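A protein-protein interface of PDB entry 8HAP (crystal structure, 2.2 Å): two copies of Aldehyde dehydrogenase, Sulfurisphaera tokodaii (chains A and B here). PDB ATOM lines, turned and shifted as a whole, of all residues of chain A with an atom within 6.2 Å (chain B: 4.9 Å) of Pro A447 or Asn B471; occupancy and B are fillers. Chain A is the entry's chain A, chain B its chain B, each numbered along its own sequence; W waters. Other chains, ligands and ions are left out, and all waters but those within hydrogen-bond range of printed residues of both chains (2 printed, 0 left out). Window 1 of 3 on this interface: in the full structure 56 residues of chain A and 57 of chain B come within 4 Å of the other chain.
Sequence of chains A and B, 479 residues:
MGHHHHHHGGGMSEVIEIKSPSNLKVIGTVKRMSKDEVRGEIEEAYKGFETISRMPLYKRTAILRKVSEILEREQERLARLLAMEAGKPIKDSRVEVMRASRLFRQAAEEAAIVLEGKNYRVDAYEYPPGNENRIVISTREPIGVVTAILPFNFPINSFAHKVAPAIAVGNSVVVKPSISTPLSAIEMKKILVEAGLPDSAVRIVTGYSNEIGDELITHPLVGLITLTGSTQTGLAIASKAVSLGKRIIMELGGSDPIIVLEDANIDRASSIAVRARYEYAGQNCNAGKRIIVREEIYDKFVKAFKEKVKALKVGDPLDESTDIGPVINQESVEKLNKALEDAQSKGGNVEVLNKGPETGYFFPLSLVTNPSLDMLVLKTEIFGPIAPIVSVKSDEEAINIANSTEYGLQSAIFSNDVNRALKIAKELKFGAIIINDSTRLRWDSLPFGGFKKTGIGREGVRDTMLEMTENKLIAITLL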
ATOM      1  N   GLN A 410       5.810 -17.247  20.869  1.00  0.00           N
ATOM      2  CA  GLN A 410       5.240 -18.561  20.489  1.00  0.00           C
ATOM      3  C   GLN A 410       3.995 -18.789  21.339  1.00  0.00           C
ATOM      4  O   GLN A 410       3.853 -18.143  22.375  1.00  0.00           O
ATOM      5  CB  GLN A 410       6.288 -19.681  20.622  1.00  0.00           C
ATOM      6  CG  GLN A 410       7.539 -19.431  19.786  1.00  0.00           C
ATOM      7  CD  GLN A 410       8.362 -20.635  19.374  1.00  0.00           C
ATOM      8  OE1 GLN A 410       8.979 -20.648  18.304  1.00  0.00           O
ATOM      9  NE2 GLN A 410       8.419 -21.644  20.228  1.00  0.00           N
ATOM     10  N   PHE A 430       1.288 -14.467  17.046  1.00  0.00           N
ATOM     11  CA  PHE A 430       2.598 -15.011  17.495  1.00  0.00           C
ATOM     12  C   PHE A 430       3.426 -15.455  16.292  1.00  0.00           C
ATOM     13  O   PHE A 430       2.843 -15.844  15.251  1.00  0.00           O
ATOM     14  CB  PHE A 430       2.423 -16.171  18.486  1.00  0.00           C
ATOM     15  CG  PHE A 430       1.686 -15.793  19.743  1.00  0.00           C
ATOM     16  CD1 PHE A 430       0.298 -15.723  19.741  1.00  0.00           C
ATOM     17  CD2 PHE A 430       2.369 -15.460  20.904  1.00  0.00           C
ATOM     18  CE1 PHE A 430      -0.392 -15.332  20.876  1.00  0.00           C
ATOM     19  CE2 PHE A 430       1.680 -15.016  22.026  1.00  0.00           C
ATOM     20  CZ  PHE A 430       0.303 -14.965  22.011  1.00  0.00           C
ATOM     21  N   GLY A 431       4.756 -15.416  16.460  1.00  0.00           N
ATOM     22  CA  GLY A 431       5.736 -15.851  15.446  1.00  0.00           C
ATOM     23  C   GLY A 431       5.657 -17.343  15.205  1.00  0.00           C
ATOM     24  O   GLY A 431       5.994 -17.780  14.103  1.00  0.00           O
ATOM     25  N   ALA A 432       5.189 -18.117  16.188  1.00  0.00           N
ATOM     26  CA  ALA A 432       4.925 -19.553  15.982  1.00  0.00           C
ATOM     27  C   ALA A 432       3.739 -19.982  16.852  1.00  0.00           C
ATOM     28  O   ALA A 432       3.594 -19.498  18.006  1.00  0.00           O
ATOM     29  CB  ALA A 432       6.185 -20.353  16.237  1.00  0.00           C
ATOM     30  N   ARG A 442      11.918 -25.219  19.467  1.00  0.00           N
ATOM     31  CA  ARG A 442      12.688 -24.342  18.535  1.00  0.00           C
ATOM     32  C   ARG A 442      13.607 -25.225  17.701  1.00  0.00           C
ATOM     33  O   ARG A 442      14.211 -26.178  18.267  1.00  0.00           O
ATOM     34  CB  ARG A 442      13.518 -23.283  19.267  1.00  0.00           C
ATOM     35  CG  ARG A 442      14.592 -22.590  18.436  1.00  0.00           C
ATOM     36  CD  ARG A 442      15.263 -21.488  19.250  1.00  0.00           C
ATOM     37  NE  ARG A 442      15.913 -20.460  18.446  1.00  0.00           N
ATOM     38  CZ  ARG A 442      16.621 -19.435  18.921  1.00  0.00           C
ATOM     39  NH1 ARG A 442      16.847 -19.279  20.215  1.00  0.00           N
ATOM     40  NH2 ARG A 442      17.096 -18.543  18.082  1.00  0.00           N
ATOM     41  N   TRP A 443      13.727 -24.877  16.423  1.00  0.00           N
ATOM     42  CA  TRP A 443      14.628 -25.512  15.443  1.00  0.00           C
ATOM     43  C   TRP A 443      15.733 -24.496  15.128  1.00  0.00           C
ATOM     44  O   TRP A 443      15.415 -23.410  14.654  1.00  0.00           O
ATOM     45  CB  TRP A 443      13.815 -25.926  14.213  1.00  0.00           C
ATOM     46  CG  TRP A 443      12.741 -26.910  14.517  1.00  0.00           C
ATOM     47  CD1 TRP A 443      12.847 -28.264  14.393  1.00  0.00           C
ATOM     48  CD2 TRP A 443      11.399 -26.644  14.980  1.00  0.00           C
ATOM     49  NE1 TRP A 443      11.683 -28.858  14.796  1.00  0.00           N
ATOM     50  CE2 TRP A 443      10.787 -27.897  15.185  1.00  0.00           C
ATOM     51  CE3 TRP A 443      10.676 -25.490  15.289  1.00  0.00           C
ATOM     52  CZ2 TRP A 443       9.472 -28.028  15.636  1.00  0.00           C
ATOM     53  CZ3 TRP A 443       9.381 -25.619  15.739  1.00  0.00           C
ATOM     54  CH2 TRP A 443       8.795 -26.868  15.920  1.00  0.00           C
ATOM     55  N   SER A 445      17.993 -24.087  12.921  1.00  0.00           N
ATOM     56  CA  SER A 445      18.096 -23.677  11.489  1.00  0.00           C
ATOM     57  C   SER A 445      16.874 -22.854  11.052  1.00  0.00           C
ATOM     58  O   SER A 445      17.010 -22.106  10.059  1.00  0.00           O
ATOM     59  CB  SER A 445      18.316 -24.857  10.553  1.00  0.00           C
ATOM     60  OG  SER A 445      19.694 -25.188  10.480  1.00  0.00           O
ATOM     61  N   LEU A 446      15.732 -22.989  11.734  1.00  0.00           N
ATOM     62  CA  LEU A 446      14.465 -22.312  11.346  1.00  0.00           C
ATOM     63  C   LEU A 446      14.397 -20.906  11.929  1.00  0.00           C
ATOM     64  O   LEU A 446      15.039 -20.575  12.950  1.00  0.00           O
ATOM     65  CB  LEU A 446      13.274 -23.152  11.804  1.00  0.00           C
ATOM     66  CG  LEU A 446      12.802 -24.215  10.804  1.00  0.00           C
ATOM     67  CD1 LEU A 446      13.887 -25.249  10.566  1.00  0.00           C
ATOM     68  CD2 LEU A 446      11.518 -24.895  11.268  1.00  0.00           C
ATOM     69  N   PRO A 447      13.544 -20.053  11.324  1.00  0.00           N
ATOM     70  CA  PRO A 447      13.216 -18.762  11.926  1.00  0.00           C
ATOM     71  C   PRO A 447      12.765 -18.973  13.385  1.00  0.00           C
ATOM     72  O   PRO A 447      12.017 -19.902  13.667  1.00  0.00           O
ATOM     73  CB  PRO A 447      12.085 -18.188  11.055  1.00  0.00           C
ATOM     74  CG  PRO A 447      12.032 -19.048   9.781  1.00  0.00           C
ATOM     75  CD  PRO A 447      12.822 -20.307  10.062  1.00  0.00           C
ATOM     76  N   PHE A 448      13.260 -18.136  14.295  1.00  0.00           N
ATOM     77  CA  PHE A 448      12.742 -18.028  15.681  1.00  0.00           C
ATOM     78  C   PHE A 448      12.610 -16.549  16.057  1.00  0.00           C
ATOM     79  O   PHE A 448      13.538 -15.759  15.739  1.00  0.00           O
ATOM     80  CB  PHE A 448      13.678 -18.733  16.655  1.00  0.00           C
ATOM     81  CG  PHE A 448      13.206 -18.730  18.087  1.00  0.00           C
ATOM     82  CD1 PHE A 448      12.237 -19.624  18.520  1.00  0.00           C
ATOM     83  CD2 PHE A 448      13.771 -17.861  19.017  1.00  0.00           C
ATOM     84  CE1 PHE A 448      11.846 -19.650  19.854  1.00  0.00           C
ATOM     85  CE2 PHE A 448      13.394 -17.891  20.352  1.00  0.00           C
ATOM     86  CZ  PHE A 448      12.420 -18.779  20.768  1.00  0.00           C
ATOM     87  N   GLY A 449      11.500 -16.177  16.697  1.00  0.00           N
ATOM     88  CA  GLY A 449      11.191 -14.761  17.000  1.00  0.00           C
ATOM     89  C   GLY A 449       9.724 -14.453  16.810  1.00  0.00           C
ATOM     90  O   GLY A 449       8.912 -15.397  16.615  1.00  0.00           O
ATOM     91  N   GLY A 450       9.349 -13.183  16.876  1.00  0.00           N
ATOM     92  CA  GLY A 450       7.917 -12.880  16.966  1.00  0.00           C
ATOM     93  C   GLY A 450       7.529 -11.504  16.501  1.00  0.00           C
ATOM     94  O   GLY A 450       8.376 -10.797  15.960  1.00  0.00           O
ATOM     95  N   PHE A 451       6.248 -11.210  16.745  1.00  0.00           N
ATOM     96  CA  PHE A 451       5.493  -9.969  16.454  1.00  0.00           C
ATOM     97  C   PHE A 451       5.758  -8.988  17.604  1.00  0.00           C
ATOM     98  O   PHE A 451       6.302  -9.417  18.666  1.00  0.00           O
ATOM     99  CB  PHE A 451       3.990 -10.296  16.356  1.00  0.00           C
ATOM    100  CG  PHE A 451       3.520 -11.162  15.205  1.00  0.00           C
ATOM    101  CD1 PHE A 451       4.261 -12.237  14.733  1.00  0.00           C
ATOM    102  CD2 PHE A 451       2.292 -10.914  14.599  1.00  0.00           C
ATOM    103  CE1 PHE A 451       3.802 -13.023  13.682  1.00  0.00           C
ATOM    104  CE2 PHE A 451       1.828 -11.705  13.552  1.00  0.00           C
ATOM    105  CZ  PHE A 451       2.587 -12.762  13.094  1.00  0.00           C
ATOM    106  N   ARG A 458      14.528 -12.327  12.656  1.00  0.00           N
ATOM    107  CA  ARG A 458      14.391 -13.714  13.139  1.00  0.00           C
ATOM    108  C   ARG A 458      15.809 -14.201  13.413  1.00  0.00           C
ATOM    109  O   ARG A 458      16.770 -13.618  12.872  1.00  0.00           O
ATOM    110  CB  ARG A 458      13.609 -14.565  12.136  1.00  0.00           C
ATOM    111  CG  ARG A 458      12.146 -14.178  12.034  1.00  0.00           C
ATOM    112  CD  ARG A 458      11.412 -14.439  13.342  1.00  0.00           C
ATOM    113  NE  ARG A 458       9.977 -14.319  13.160  1.00  0.00           N
ATOM    114  CZ  ARG A 458       9.271 -13.191  13.275  1.00  0.00           C
ATOM    115  NH1 ARG A 458       9.862 -12.034  13.564  1.00  0.00           N
ATOM    116  NH2 ARG A 458       7.963 -13.230  13.069  1.00  0.00           N
ATOM    117  N   GLU A 459      15.941 -15.195  14.272  1.00  0.00           N
ATOM    118  CA  GLU A 459      17.269 -15.766  14.580  1.00  0.00           C
ATOM    119  C   GLU A 459      17.195 -17.267  14.340  1.00  0.00           C
ATOM    120  O   GLU A 459      16.363 -17.922  14.918  1.00  0.00           O
ATOM    121  CB  GLU A 459      17.723 -15.399  15.991  1.00  0.00           C
ATOM    122  CG  GLU A 459      19.073 -16.006  16.342  1.00  0.00           C
ATOM    123  CD  GLU A 459      19.610 -15.633  17.710  1.00  0.00           C
ATOM    124  OE1 GLU A 459      20.551 -14.783  17.754  1.00  0.00           O
ATOM    125  OE2 GLU A 459      19.081 -16.183  18.727  1.00  0.00           O
ATOM    126  N   GLY A 460      18.078 -17.757  13.487  1.00  0.00           N
ATOM    127  CA  GLY A 460      18.204 -19.173  13.123  1.00  0.00           C
ATOM    128  C   GLY A 460      19.255 -19.217  12.057  1.00  0.00           C
ATOM    129  O   GLY A 460      19.417 -18.151  11.391  1.00  0.00           O
ATOM    130  N   ASP A 463      18.223 -17.670   8.612  1.00  0.00           N
ATOM    131  CA  ASP A 463      17.764 -16.254   8.644  1.00  0.00           C
ATOM    132  C   ASP A 463      18.891 -15.357   9.170  1.00  0.00           C
ATOM    133  O   ASP A 463      19.103 -14.255   8.612  1.00  0.00           O
ATOM    134  CB  ASP A 463      16.448 -16.130   9.401  1.00  0.00           C
ATOM    135  CG  ASP A 463      15.245 -16.484   8.531  1.00  0.00           C
ATOM    136  OD1 ASP A 463      15.042 -17.686   8.244  1.00  0.00           O
ATOM    137  OD2 ASP A 463      14.539 -15.554   8.121  1.00  0.00           O
ATOM    138  N   TYR B 120       8.810 -27.262   6.165  1.00  0.00           N
ATOM    139  CA  TYR B 120      10.198 -27.554   6.615  1.00  0.00           C
ATOM    140  C   TYR B 120      10.405 -29.062   6.779  1.00  0.00           C
ATOM    141  O   TYR B 120       9.513 -29.795   7.295  1.00  0.00           O
ATOM    142  CB  TYR B 120      10.496 -26.815   7.919  1.00  0.00           C
ATOM    143  CG  TYR B 120      10.612 -25.328   7.734  1.00  0.00           C
ATOM    144  CD1 TYR B 120      11.776 -24.808   7.205  1.00  0.00           C
ATOM    145  CD2 TYR B 120       9.608 -24.442   8.085  1.00  0.00           C
ATOM    146  CE1 TYR B 120      11.953 -23.456   7.022  1.00  0.00           C
ATOM    147  CE2 TYR B 120       9.764 -23.073   7.886  1.00  0.00           C
ATOM    148  CZ  TYR B 120      10.952 -22.579   7.361  1.00  0.00           C
ATOM    149  OH  TYR B 120      11.235 -21.255   7.149  1.00  0.00           O
ATOM    150  N   SER B 138       5.243 -22.458   7.273  1.00  0.00           N
ATOM    151  CA  SER B 138       5.406 -21.001   7.437  1.00  0.00           C
ATOM    152  C   SER B 138       4.433 -20.287   6.496  1.00  0.00           C
ATOM    153  O   SER B 138       4.087 -20.832   5.436  1.00  0.00           O
ATOM    154  CB  SER B 138       6.846 -20.607   7.215  1.00  0.00           C
ATOM    155  OG  SER B 138       7.176 -20.641   5.835  1.00  0.00           O
ATOM    156  N   THR B 139       3.967 -19.130   6.926  1.00  0.00           N
ATOM    157  CA  THR B 139       3.133 -18.185   6.148  1.00  0.00           C
ATOM    158  C   THR B 139       3.670 -16.782   6.410  1.00  0.00           C
ATOM    159  O   THR B 139       4.264 -16.551   7.494  1.00  0.00           O
ATOM    160  CB  THR B 139       1.648 -18.182   6.548  1.00  0.00           C
ATOM    161  OG1 THR B 139       1.608 -17.607   7.857  1.00  0.00           O
ATOM    162  CG2 THR B 139       0.982 -19.541   6.578  1.00  0.00           C
ATOM    163  N   ARG B 140       3.405 -15.872   5.488  1.00  0.00           N
ATOM    164  CA  ARG B 140       3.756 -14.445   5.618  1.00  0.00           C
ATOM    165  C   ARG B 140       2.502 -13.679   6.035  1.00  0.00           C
ATOM    166  O   ARG B 140       1.523 -13.659   5.261  1.00  0.00           O
ATOM    167  CB  ARG B 140       4.373 -14.007   4.292  1.00  0.00           C
ATOM    168  CG  ARG B 140       5.761 -14.592   4.085  1.00  0.00           C
ATOM    169  CD  ARG B 140       6.744 -13.469   4.334  1.00  0.00           C
ATOM    170  NE  ARG B 140       7.927 -14.007   4.915  1.00  0.00           N
ATOM    171  CZ  ARG B 140       8.749 -13.352   5.699  1.00  0.00           C
ATOM    172  NH1 ARG B 140       8.546 -12.079   6.007  1.00  0.00           N
ATOM    173  NH2 ARG B 140       9.777 -14.018   6.189  1.00  0.00           N
ATOM    174  N   THR B 469       5.888  -8.056   5.918  1.00  0.00           N
ATOM    175  CA  THR B 469       5.175  -9.217   6.496  1.00  0.00           C
ATOM    176  C   THR B 469       6.010  -9.806   7.638  1.00  0.00           C
ATOM    177  O   THR B 469       7.199  -9.502   7.722  1.00  0.00           O
ATOM    178  CB  THR B 469       4.834 -10.262   5.429  1.00  0.00           C
ATOM    179  OG1 THR B 469       6.019 -10.538   4.687  1.00  0.00           O
ATOM    180  CG2 THR B 469       3.761  -9.775   4.482  1.00  0.00           C
ATOM    181  N   GLU B 470       5.343 -10.535   8.531  1.00  0.00           N
ATOM    182  CA  GLU B 470       5.974 -11.342   9.603  1.00  0.00           C
ATOM    183  C   GLU B 470       5.880 -12.810   9.190  1.00  0.00           C
ATOM    184  O   GLU B 470       4.795 -13.257   8.779  1.00  0.00           O
ATOM    185  CB  GLU B 470       5.268 -11.119  10.942  1.00  0.00           C
ATOM    186  CG  GLU B 470       5.384  -9.697  11.486  1.00  0.00           C
ATOM    187  CD  GLU B 470       6.614  -9.324  12.312  1.00  0.00           C
ATOM    188  OE1 GLU B 470       7.258 -10.222  12.912  1.00  0.00           O
ATOM    189  OE2 GLU B 470       6.913  -8.113  12.378  1.00  0.00           O
ATOM    190  N   ASN B 471       6.993 -13.521   9.286  1.00  0.00           N
ATOM    191  CA  ASN B 471       7.017 -14.997   9.254  1.00  0.00           C
ATOM    192  C   ASN B 471       6.202 -15.546  10.427  1.00  0.00           C
ATOM    193  O   ASN B 471       6.395 -15.099  11.588  1.00  0.00           O
ATOM    194  CB  ASN B 471       8.440 -15.529   9.329  1.00  0.00           C
ATOM    195  CG  ASN B 471       8.534 -16.941   8.800  1.00  0.00           C
ATOM    196  OD1 ASN B 471       8.601 -17.898   9.575  1.00  0.00           O
ATOM    197  ND2 ASN B 471       8.457 -17.074   7.495  1.00  0.00           N
ATOM    198  N   LYS B 472       5.317 -16.493  10.162  1.00  0.00           N
ATOM    199  CA  LYS B 472       4.570 -17.196  11.235  1.00  0.00           C
ATOM    200  C   LYS B 472       4.682 -18.698  10.974  1.00  0.00           C
ATOM    201  O   LYS B 472       4.316 -19.129   9.862  1.00  0.00           O
ATOM    202  CB  LYS B 472       3.129 -16.699  11.285  1.00  0.00           C
ATOM    203  CG  LYS B 472       2.201 -17.376  12.288  1.00  0.00           C
ATOM    204  CD  LYS B 472       0.895 -16.618  12.378  1.00  0.00           C
ATOM    205  CE  LYS B 472      -0.179 -17.347  13.142  1.00  0.00           C
ATOM    206  NZ  LYS B 472      -1.378 -16.490  13.242  1.00  0.00           N
ATOM    207  N   LEU B 473       5.251 -19.437  11.931  1.00  0.00           N
ATOM    208  CA  LEU B 473       5.323 -20.917  11.868  1.00  0.00           C
ATOM    209  C   LEU B 473       4.042 -21.507  12.471  1.00  0.00           C
ATOM    210  O   LEU B 473       3.548 -20.971  13.452  1.00  0.00           O
ATOM    211  CB  LEU B 473       6.564 -21.407  12.621  1.00  0.00           C
ATOM    212  CG  LEU B 473       7.788 -21.747  11.771  1.00  0.00           C
ATOM    213  CD1 LEU B 473       8.170 -20.640  10.819  1.00  0.00           C
ATOM    214  CD2 LEU B 473       8.973 -22.091  12.663  1.00  0.00           C
HETATM  215  O   HOH W   1      14.197 -20.601   6.665  1.00  0.00           O
HETATM  216  O   HOH W   2       8.430 -16.983  12.683  1.00  0.00           O
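No position is printed for both chains.
Phe A430 touches Lys B472.
O of Gly A431 touches O of Asn B471, at 3.7 Å.
Gly A431 touches Lys B472.
Ala A432 touches Leu B473.
Tyr B120 touches Leu A446.
OH of Tyr B120 touches CD of Pro A447, at 3.5 Å.
Asn B471 touches Pro A447 (OD1 to CG, 3.6 Å).
Leu B473 touches Pro A447.
Phe A451 touches Glu B470 (CE1 to CB, 3.6 Å).
Phe A451 touches Asn B471.
Pro A447 touches just these residues of chain B: Tyr B120, Asn B471 and Leu B473.
Asn B471 touches just these residues of chain A: Gly A431, Pro A447, Phe A451 and Arg A458.
Printed residues of chain B within 4 Å of Phe A451: Glu B470 (3.6 Å) and Asn B471 (3.9 Å).
Printed residues of chain B within 4 Å of Phe A430: Lys B472.
Of the printed residues of chain A, Lys B472 touches Phe A430 (3.4 Å) and Gly A431 (3.3 Å).
Printed residues of chain A within 4 Å of Glu B470: Gly A450 (3.3 Å), Phe A451 (3.6 Å) and Arg A458 (3.1 Å).
Printed residues of chain A within 4 Å of Tyr B120: Leu A446 (3.7 Å) and Pro A447 (3.5 Å).
Of the 17 printed residues of chain A, 8 touch a printed residue of chain B.
Hydrophobic or aromatic side chains of chain A that line the printed part of chain B: Ala A432, Leu A446, Pro A447 and Phe A451.
Printed residues of chain B that touch a printed residue of chain A: Tyr B120, Glu B470, Asn B471, Lys B472 and Leu B473.
Hydrophobic or aromatic side chains of chain B within 4 Å of the printed part of chain A: Tyr B120 and Leu B473.
Among the printed residues, 14 pairs touch across the chains.
Among the printed residues, Asp or Glu carboxylates within 4 Å of a Lys or Arg side-chain nitrogen of the other chain: Arg A458 with Glu B470.
The backbone NH of Leu B473 lies within hydrogen-bond range of the backbone carbonyl oxygen of Gly A431, 2.8 Å away.
The side-chain carboxylate (OE1) of Glu B470 lies within salt-bridge range of the guanidinium group (NH2) of Arg A458, 3.1 Å away.
O of Asn B471 sits at hydrogen-bond distance from NH2 of Arg A458, 2.9 Å away.
The side-chain carboxylate (OE1) of Glu B470 sits close to the backbone carbonyl oxygen (O) of Gly A450 (3.3 Å).
The guanidinium group (NH1) of Arg A458 lies within hydrogen-bond range of the backbone carbonyl oxygen (O) of Gly A450 (3.1 Å).
N of Lys B472 is in hydrogen-bond range of O of Thr B139 (2.9 Å).
Water W2 lies within hydrogen-bond range of the backbone carbonyl oxygen (O) of Gly A431 (2.9 Å), the backbone carbonyl oxygen (O) of Asn B471 (3.0 Å) and the guanidinium group (NE) of Arg A458 (3.1 Å).
Water W1 bridges OH of Tyr B120 (3.1 Å) and OD1 of Asp A463 (3.4 Å).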
